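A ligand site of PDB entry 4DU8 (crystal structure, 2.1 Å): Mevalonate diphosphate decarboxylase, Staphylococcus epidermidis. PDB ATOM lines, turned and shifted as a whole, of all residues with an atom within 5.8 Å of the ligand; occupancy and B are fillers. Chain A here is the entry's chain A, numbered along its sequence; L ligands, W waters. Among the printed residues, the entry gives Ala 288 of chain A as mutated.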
ATOM      1  N   ASN A  17      19.256  -2.873   7.539  1.00  0.00           N
ATOM      2  CA  ASN A  17      18.927  -4.287   7.617  1.00  0.00           C
ATOM      3  C   ASN A  17      19.551  -4.842   8.888  1.00  0.00           C
ATOM      4  O   ASN A  17      20.613  -4.363   9.332  1.00  0.00           O
ATOM      5  CB  ASN A  17      19.455  -5.036   6.397  1.00  0.00           C
ATOM      6  CG  ASN A  17      20.970  -5.161   6.403  1.00  0.00           C
ATOM      7  OD1 ASN A  17      21.519  -5.971   7.137  1.00  0.00           O
ATOM      8  ND2 ASN A  17      21.647  -4.343   5.601  1.00  0.00           N
ATOM      9  N   ALA A  19      21.034  -8.319  10.633  1.00  0.00           N
ATOM     10  CA  ALA A  19      21.569  -9.651  10.355  1.00  0.00           C
ATOM     11  C   ALA A  19      20.920 -10.679  11.258  1.00  0.00           C
ATOM     12  O   ALA A  19      20.965 -10.534  12.476  1.00  0.00           O
ATOM     13  CB  ALA A  19      23.090  -9.669  10.563  1.00  0.00           C
ATOM     14  N   ILE A  21      21.566 -14.207  10.557  1.00  0.00           N
ATOM     15  CA  ILE A  21      22.782 -14.986  10.686  1.00  0.00           C
ATOM     16  C   ILE A  21      23.917 -13.976  10.552  1.00  0.00           C
ATOM     17  O   ILE A  21      24.027 -13.283   9.540  1.00  0.00           O
ATOM     18  CB  ILE A  21      22.901 -16.094   9.634  1.00  0.00           C
ATOM     19  CG1 ILE A  21      21.708 -17.043   9.720  1.00  0.00           C
ATOM     20  CG2 ILE A  21      24.183 -16.865   9.835  1.00  0.00           C
ATOM     21  CD1 ILE A  21      21.760 -17.984  10.933  1.00  0.00           C
ATOM     22  N   LYS A  22      24.754 -13.903  11.576  1.00  0.00           N
ATOM     23  CA  LYS A  22      25.681 -12.796  11.727  1.00  0.00           C
ATOM     24  C   LYS A  22      26.878 -12.903  10.797  1.00  0.00           C
ATOM     25  O   LYS A  22      27.441 -13.992  10.559  1.00  0.00           O
ATOM     26  CB  LYS A  22      26.165 -12.713  13.175  1.00  0.00           C
ATOM     27  CG  LYS A  22      25.045 -12.687  14.222  1.00  0.00           C
ATOM     28  CD  LYS A  22      24.216 -11.397  14.092  1.00  0.00           C
ATOM     29  CE  LYS A  22      23.333 -11.162  15.306  1.00  0.00           C
ATOM     30  NZ  LYS A  22      22.441  -9.980  15.107  1.00  0.00           N
ATOM     31  N   TYR A  23      27.244 -11.757  10.242  1.00  0.00           N
ATOM     32  CA  TYR A  23      28.577 -11.541   9.704  1.00  0.00           C
ATOM     33  C   TYR A  23      29.395 -11.111  10.915  1.00  0.00           C
ATOM     34  O   TYR A  23      28.986 -10.228  11.652  1.00  0.00           O
ATOM     35  CB  TYR A  23      28.494 -10.450   8.623  1.00  0.00           C
ATOM     36  CG  TYR A  23      29.654  -9.469   8.536  1.00  0.00           C
ATOM     37  CD1 TYR A  23      30.957  -9.908   8.337  1.00  0.00           C
ATOM     38  CD2 TYR A  23      29.423  -8.104   8.623  1.00  0.00           C
ATOM     39  CE1 TYR A  23      32.010  -9.000   8.249  1.00  0.00           C
ATOM     40  CE2 TYR A  23      30.453  -7.198   8.534  1.00  0.00           C
ATOM     41  CZ  TYR A  23      31.742  -7.647   8.348  1.00  0.00           C
ATOM     42  OH  TYR A  23      32.758  -6.731   8.259  1.00  0.00           O
ATOM     43  N   TRP A  24      30.535 -11.743  11.135  1.00  0.00           N
ATOM     44  CA  TRP A  24      31.368 -11.388  12.280  1.00  0.00           C
ATOM     45  C   TRP A  24      32.778 -11.904  12.054  1.00  0.00           C
ATOM     46  O   TRP A  24      33.037 -13.103  12.194  1.00  0.00           O
ATOM     47  CB  TRP A  24      30.778 -11.972  13.562  1.00  0.00           C
ATOM     48  CG  TRP A  24      31.369 -11.385  14.821  1.00  0.00           C
ATOM     49  CD1 TRP A  24      32.128 -12.038  15.756  1.00  0.00           C
ATOM     50  CD2 TRP A  24      31.251 -10.043  15.270  1.00  0.00           C
ATOM     51  NE1 TRP A  24      32.474 -11.168  16.764  1.00  0.00           N
ATOM     52  CE2 TRP A  24      31.961  -9.942  16.481  1.00  0.00           C
ATOM     53  CE3 TRP A  24      30.629  -8.907  14.759  1.00  0.00           C
ATOM     54  CZ2 TRP A  24      32.055  -8.747  17.191  1.00  0.00           C
ATOM     55  CZ3 TRP A  24      30.724  -7.720  15.463  1.00  0.00           C
ATOM     56  CH2 TRP A  24      31.423  -7.655  16.671  1.00  0.00           C
ATOM     57  N   LYS A  26      36.409 -10.732   9.411  1.00  0.00           N
ATOM     58  CA  LYS A  26      36.742 -10.552   7.997  1.00  0.00           C
ATOM     59  C   LYS A  26      37.891 -11.450   7.551  1.00  0.00           C
ATOM     60  O   LYS A  26      38.865 -11.635   8.282  1.00  0.00           O
ATOM     61  CB  LYS A  26      37.147  -9.094   7.725  1.00  0.00           C
ATOM     62  CG  LYS A  26      36.105  -8.013   8.045  1.00  0.00           C
ATOM     63  CD  LYS A  26      36.548  -6.647   7.519  1.00  0.00           C
ATOM     64  CE  LYS A  26      36.251  -5.505   8.468  1.00  0.00           C
ATOM     65  NZ  LYS A  26      34.983  -5.654   9.243  1.00  0.00           N
ATOM     66  N   ILE A  32      37.072  -5.630   2.621  1.00  0.00           N
ATOM     67  CA  ILE A  32      35.951  -6.076   3.433  1.00  0.00           C
ATOM     68  C   ILE A  32      35.351  -7.363   2.873  1.00  0.00           C
ATOM     69  O   ILE A  32      34.225  -7.382   2.380  1.00  0.00           O
ATOM     70  CB  ILE A  32      34.898  -4.951   3.632  1.00  0.00           C
ATOM     71  CG1 ILE A  32      35.569  -3.718   4.251  1.00  0.00           C
ATOM     72  CG2 ILE A  32      33.764  -5.422   4.514  1.00  0.00           C
ATOM     73  CD1 ILE A  32      34.640  -2.546   4.438  1.00  0.00           C
ATOM     74  N   SER A  38      26.214 -14.184   5.488  1.00  0.00           N
ATOM     75  CA  SER A  38      25.272 -13.630   6.450  1.00  0.00           C
ATOM     76  C   SER A  38      23.897 -13.524   5.832  1.00  0.00           C
ATOM     77  O   SER A  38      23.757 -13.523   4.612  1.00  0.00           O
ATOM     78  CB  SER A  38      25.735 -12.266   6.977  1.00  0.00           C
ATOM     79  OG  SER A  38      25.960 -11.350   5.909  1.00  0.00           O
ATOM     80  N   SER A 112      25.402   2.560   9.148  1.00  0.00           N
ATOM     81  CA  SER A 112      26.412   2.345   8.110  1.00  0.00           C
ATOM     82  C   SER A 112      25.828   1.559   6.932  1.00  0.00           C
ATOM     83  O   SER A 112      26.129   1.858   5.786  1.00  0.00           O
ATOM     84  CB  SER A 112      27.670   1.657   8.670  1.00  0.00           C
ATOM     85  OG  SER A 112      27.396   0.330   9.079  1.00  0.00           O
ATOM     86  N   GLY A 143      32.311   0.098   1.445  1.00  0.00           N
ATOM     87  CA  GLY A 143      32.112   1.167   2.414  1.00  0.00           C
ATOM     88  C   GLY A 143      31.848   0.572   3.772  1.00  0.00           C
ATOM     89  O   GLY A 143      32.448   0.965   4.782  1.00  0.00           O
ATOM     90  N   SER A 144      30.970  -0.424   3.791  1.00  0.00           N
ATOM     91  CA  SER A 144      30.677  -1.153   5.020  1.00  0.00           C
ATOM     92  C   SER A 144      30.039  -2.488   4.668  1.00  0.00           C
ATOM     93  O   SER A 144      29.086  -2.543   3.883  1.00  0.00           O
ATOM     94  CB  SER A 144      29.763  -0.322   5.917  1.00  0.00           C
ATOM     95  OG  SER A 144      29.545  -0.973   7.153  1.00  0.00           O
ATOM     96  N   GLY A 145      30.552  -3.563   5.248  1.00  0.00           N
ATOM     97  CA  GLY A 145      30.108  -4.912   4.900  1.00  0.00           C
ATOM     98  C   GLY A 145      28.612  -5.085   4.910  1.00  0.00           C
ATOM     99  O   GLY A 145      28.024  -5.574   3.939  1.00  0.00           O
ATOM    100  N   SER A 146      27.962  -4.686   5.996  1.00  0.00           N
ATOM    101  CA  SER A 146      26.510  -4.833   6.100  1.00  0.00           C
ATOM    102  C   SER A 146      25.765  -4.048   5.006  1.00  0.00           C
ATOM    103  O   SER A 146      24.628  -4.368   4.672  1.00  0.00           O
ATOM    104  CB  SER A 146      26.034  -4.383   7.470  1.00  0.00           C
ATOM    105  OG  SER A 146      26.452  -3.054   7.717  1.00  0.00           O
ATOM    106  N   ALA A 147      26.382  -3.017   4.454  1.00  0.00           N
ATOM    107  CA  ALA A 147      25.699  -2.228   3.420  1.00  0.00           C
ATOM    108  C   ALA A 147      25.453  -3.035   2.140  1.00  0.00           C
ATOM    109  O   ALA A 147      24.538  -2.721   1.352  1.00  0.00           O
ATOM    110  CB  ALA A 147      26.469  -0.972   3.102  1.00  0.00           C
ATOM    111  N   ARG A 149      24.043  -5.692   1.823  1.00  0.00           N
ATOM    112  CA  ARG A 149      22.736  -6.356   1.897  1.00  0.00           C
ATOM    113  C   ARG A 149      21.583  -5.375   1.767  1.00  0.00           C
ATOM    114  O   ARG A 149      20.493  -5.744   1.353  1.00  0.00           O
ATOM    115  CB  ARG A 149      22.604  -7.154   3.205  1.00  0.00           C
ATOM    116  CG  ARG A 149      23.816  -8.071   3.484  1.00  0.00           C
ATOM    117  CD  ARG A 149      23.608  -8.933   4.729  1.00  0.00           C
ATOM    118  NE  ARG A 149      23.372  -8.126   5.918  1.00  0.00           N
ATOM    119  CZ  ARG A 149      24.217  -8.029   6.927  1.00  0.00           C
ATOM    120  NH1 ARG A 149      25.345  -8.722   6.911  1.00  0.00           N
ATOM    121  NH2 ARG A 149      23.919  -7.250   7.965  1.00  0.00           N
ATOM    122  N   TRP A 158      24.433 -12.243   2.076  1.00  0.00           N
ATOM    123  CA  TRP A 158      25.738 -11.827   1.596  1.00  0.00           C
ATOM    124  C   TRP A 158      26.599 -13.065   1.367  1.00  0.00           C
ATOM    125  O   TRP A 158      26.950 -13.789   2.296  1.00  0.00           O
ATOM    126  CB  TRP A 158      26.363 -10.891   2.612  1.00  0.00           C
ATOM    127  CG  TRP A 158      27.698 -10.402   2.301  1.00  0.00           C
ATOM    128  CD1 TRP A 158      28.398 -10.572   1.135  1.00  0.00           C
ATOM    129  CD2 TRP A 158      28.547  -9.671   3.177  1.00  0.00           C
ATOM    130  NE1 TRP A 158      29.626  -9.971   1.231  1.00  0.00           N
ATOM    131  CE2 TRP A 158      29.748  -9.412   2.478  1.00  0.00           C
ATOM    132  CE3 TRP A 158      28.409  -9.198   4.485  1.00  0.00           C
ATOM    133  CZ2 TRP A 158      30.796  -8.707   3.053  1.00  0.00           C
ATOM    134  CZ3 TRP A 158      29.458  -8.502   5.054  1.00  0.00           C
ATOM    135  CH2 TRP A 158      30.634  -8.256   4.335  1.00  0.00           C
ATOM    136  N   SER A 197      32.337  -1.814  16.209  1.00  0.00           N
ATOM    137  CA  SER A 197      32.078  -3.077  15.533  1.00  0.00           C
ATOM    138  C   SER A 197      33.251  -3.685  14.749  1.00  0.00           C
ATOM    139  O   SER A 197      33.631  -4.846  14.963  1.00  0.00           O
ATOM    140  CB  SER A 197      30.868  -2.936  14.605  1.00  0.00           C
ATOM    141  OG  SER A 197      30.506  -4.206  14.082  1.00  0.00           O
ATOM    142  N   ARG A 198      33.823  -2.899  13.830  1.00  0.00           N
ATOM    143  CA  ARG A 198      34.944  -3.344  12.993  1.00  0.00           C
ATOM    144  C   ARG A 198      36.115  -3.800  13.841  1.00  0.00           C
ATOM    145  O   ARG A 198      36.805  -4.770  13.505  1.00  0.00           O
ATOM    146  CB  ARG A 198      35.386  -2.205  12.047  1.00  0.00           C
ATOM    147  CG  ARG A 198      36.652  -2.482  11.221  1.00  0.00           C
ATOM    148  CD  ARG A 198      36.842  -1.402  10.118  1.00  0.00           C
ATOM    149  NE  ARG A 198      35.682  -1.312   9.222  1.00  0.00           N
ATOM    150  CZ  ARG A 198      35.547  -0.435   8.232  1.00  0.00           C
ATOM    151  NH1 ARG A 198      36.497   0.458   7.985  1.00  0.00           N
ATOM    152  NH2 ARG A 198      34.453  -0.441   7.474  1.00  0.00           N
ATOM    153  N   MET A 201      35.168  -7.264  16.152  1.00  0.00           N
ATOM    154  CA  MET A 201      35.122  -8.509  15.400  1.00  0.00           C
ATOM    155  C   MET A 201      36.533  -8.887  14.949  1.00  0.00           C
ATOM    156  O   MET A 201      36.861 -10.077  14.801  1.00  0.00           O
ATOM    157  CB  MET A 201      34.175  -8.395  14.201  1.00  0.00           C
ATOM    158  CG  MET A 201      34.767  -7.672  13.002  1.00  0.00           C
ATOM    159  SD  MET A 201      33.730  -7.781  11.523  1.00  0.00           S
ATOM    160  CE  MET A 201      32.176  -7.067  12.060  1.00  0.00           C
ATOM    161  N   MET A 248      27.632 -16.090  18.197  1.00  0.00           N
ATOM    162  CA  MET A 248      28.439 -14.956  17.761  1.00  0.00           C
ATOM    163  C   MET A 248      28.972 -14.206  18.982  1.00  0.00           C
ATOM    164  O   MET A 248      30.143 -13.848  19.051  1.00  0.00           O
ATOM    165  CB  MET A 248      27.634 -14.007  16.862  1.00  0.00           C
ATOM    166  CG  MET A 248      28.501 -12.921  16.185  1.00  0.00           C
ATOM    167  SD  MET A 248      27.669 -11.323  16.064  1.00  0.00           S
ATOM    168  CE  MET A 248      28.086 -10.615  17.668  1.00  0.00           C
ATOM    169  N   MET A 287      21.236  -9.786  18.775  1.00  0.00           N
ATOM    170  CA  MET A 287      21.916  -8.580  19.219  1.00  0.00           C
ATOM    171  C   MET A 287      23.117  -8.326  18.312  1.00  0.00           C
ATOM    172  O   MET A 287      23.777  -9.284  17.897  1.00  0.00           O
ATOM    173  CB  MET A 287      22.419  -8.722  20.662  1.00  0.00           C
ATOM    174  CG  MET A 287      21.335  -8.716  21.729  1.00  0.00           C
ATOM    175  SD  MET A 287      20.477 -10.292  21.912  1.00  0.00           S
ATOM    176  CE  MET A 287      21.840 -11.443  22.098  1.00  0.00           C
ATOM    177  N   ALA A 288      23.420  -7.066  18.026  1.00  0.00           N
ATOM    178  CA  ALA A 288      24.572  -6.726  17.197  1.00  0.00           C
ATOM    179  C   ALA A 288      25.775  -6.356  18.065  1.00  0.00           C
ATOM    180  O   ALA A 288      26.045  -6.998  19.073  1.00  0.00           O
ATOM    181  CB  ALA A 288      24.228  -5.595  16.240  1.00  0.00           C
ATOM    182  N   ALA A 289      26.485  -5.314  17.676  1.00  0.00           N
ATOM    183  CA  ALA A 289      27.667  -4.865  18.423  1.00  0.00           C
ATOM    184  C   ALA A 289      27.291  -3.856  19.501  1.00  0.00           C
ATOM    185  O   ALA A 289      27.837  -2.757  19.554  1.00  0.00           O
ATOM    186  CB  ALA A 289      28.715  -4.281  17.463  1.00  0.00           C
HETATM  187  C1  LIG L   1      26.143  -7.596  10.618  1.00  0.00           C
HETATM  188  N1  LIG L   1      27.206  -6.835  12.771  1.00  0.00           N
HETATM  189  O1  LIG L   1      25.543  -6.478  10.533  1.00  0.00           O
HETATM  190  C2  LIG L   1      27.013  -7.945  11.844  1.00  0.00           C
HETATM  191  C3  LIG L   1      26.426  -9.077  12.588  1.00  0.00           C
HETATM  192  C4  LIG L   1      26.458  -7.104  13.968  1.00  0.00           C
HETATM  193  C5  LIG L   1      26.264  -8.595  14.005  1.00  0.00           C
HETATM  194  O2  LIG L   1      28.077  -4.779  13.447  1.00  0.00           O
HETATM  195  O3  LIG L   1      31.851  -2.006   8.192  1.00  0.00           O
HETATM  196  O4  LIG L   1      29.137  -3.908   8.651  1.00  0.00           O
HETATM  197  O5  LIG L   1      33.703  -3.256   9.342  1.00  0.00           O
HETATM  198  O6  LIG L   1      32.217  -4.408   7.690  1.00  0.00           O
HETATM  199  O7  LIG L   1      29.609  -1.833   9.961  1.00  0.00           O
HETATM  200  C6  LIG L   1      28.771  -5.398  11.307  1.00  0.00           C
HETATM  201  O8  LIG L   1      29.041  -3.985  11.183  1.00  0.00           O
HETATM  202  O9  LIG L   1      31.311  -3.710   9.978  1.00  0.00           O
HETATM  203  C7  LIG L   1      28.015  -5.622  12.561  1.00  0.00           C
HETATM  204  P1  LIG L   1      32.294  -3.336   8.797  1.00  0.00           P
HETATM  205  P2  LIG L   1      29.766  -3.359   9.919  1.00  0.00           P
HETATM  206  O10 LIG L   1      26.001  -8.449   9.678  1.00  0.00           O
HETATM  207  O   HOH W   1      26.217  -3.482  15.473  1.00  0.00           O
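Water W1 lies within hydrogen-bond range of the backbone NH (N) of Ala 289 (2.9 Å) and an oxygen (O2) of the ligand (3.0 Å).
The side-chain hydroxyl of Tyr 23 lies within hydrogen-bond range of the side-chain amino group of Lys 26 (2.7 Å).
The side-chain hydroxyl of Tyr 23 lies within hydrogen-bond range of the side-chain sulfur of Met 201.
The side-chain amino group of Lys 26 is in hydrogen-bond range of the side-chain sulfur of Met 201 (3.4 Å).
OG of Ser 112 sits at hydrogen-bond distance from OG of Ser 144 (3.2 Å).
NH1 of Arg 149 sits at hydrogen-bond distance from OG of Ser 38 (2.9 Å).
ND2 of Asn 17 is in hydrogen-bond range of O of Ser 146, at 3.1 Å.
O of Ala 19 lies within hydrogen-bond range of NZ of Lys 22 (3.1 Å).
The backbone carbonyl oxygen (O) of Met 287 sits at hydrogen-bond distance from the side-chain amino group (NZ) of Lys 22 (3.2 Å).
Residues that only touch the ligand: Ala 19, Lys 22, Ala 288, Ile 32, Met 248 and Met 201.
Hydrophobic or aromatic side chains within 4 Å of the ligand: Ala 19, Tyr 23, Ile 32, Met 201, Met 248 and Ala 288.
Within 4 Å of the ligand: Ala 19, Lys 22, Tyr 23, Lys 26, Ile 32, Ser 112, Ser 144, Gly 145, Ser 146, Arg 149, Ser 197, Arg 198, Met 201, Met 248 and Ala 288.
The nearest printed residue that does not touch the ligand is Ala 289 (4.1 Å).
An oxygen (O6) of the ligand lies within hydrogen-bond range of the side-chain hydroxyl (OH) of Tyr 23 (2.5 Å).
OG of Ser 197 lies within hydrogen-bond range of O2 of the ligand, 2.6 Å away.
NZ of Lys 26 is in salt-bridge range of O5 of the ligand, 2.7 Å away.
An oxygen (O3) of the ligand is in hydrogen-bond range of the side-chain hydroxyl (OG) of Ser 144 (2.7 Å).
The guanidinium group (NE) of Arg 198 lies within salt-bridge range of an oxygen (O5) of the ligand, 2.8 Å away.
An oxygen (O10) of the ligand lies within salt-bridge range of the guanidinium group (NH1) of Arg 149 (2.9 Å).
The backbone NH (N) of Ser 146 is in hydrogen-bond range of an oxygen (O4) of the ligand, at 3.0 Å.
OG of Ser 146 sits at hydrogen-bond distance from O4 of the ligand (3.0 Å).
The backbone NH of Gly 145 sits at hydrogen-bond distance from an oxygen (O6) of the ligand, at 3.1 Å.
OG of Ser 112 lies within hydrogen-bond range of O7 of the ligand (3.2 Å).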
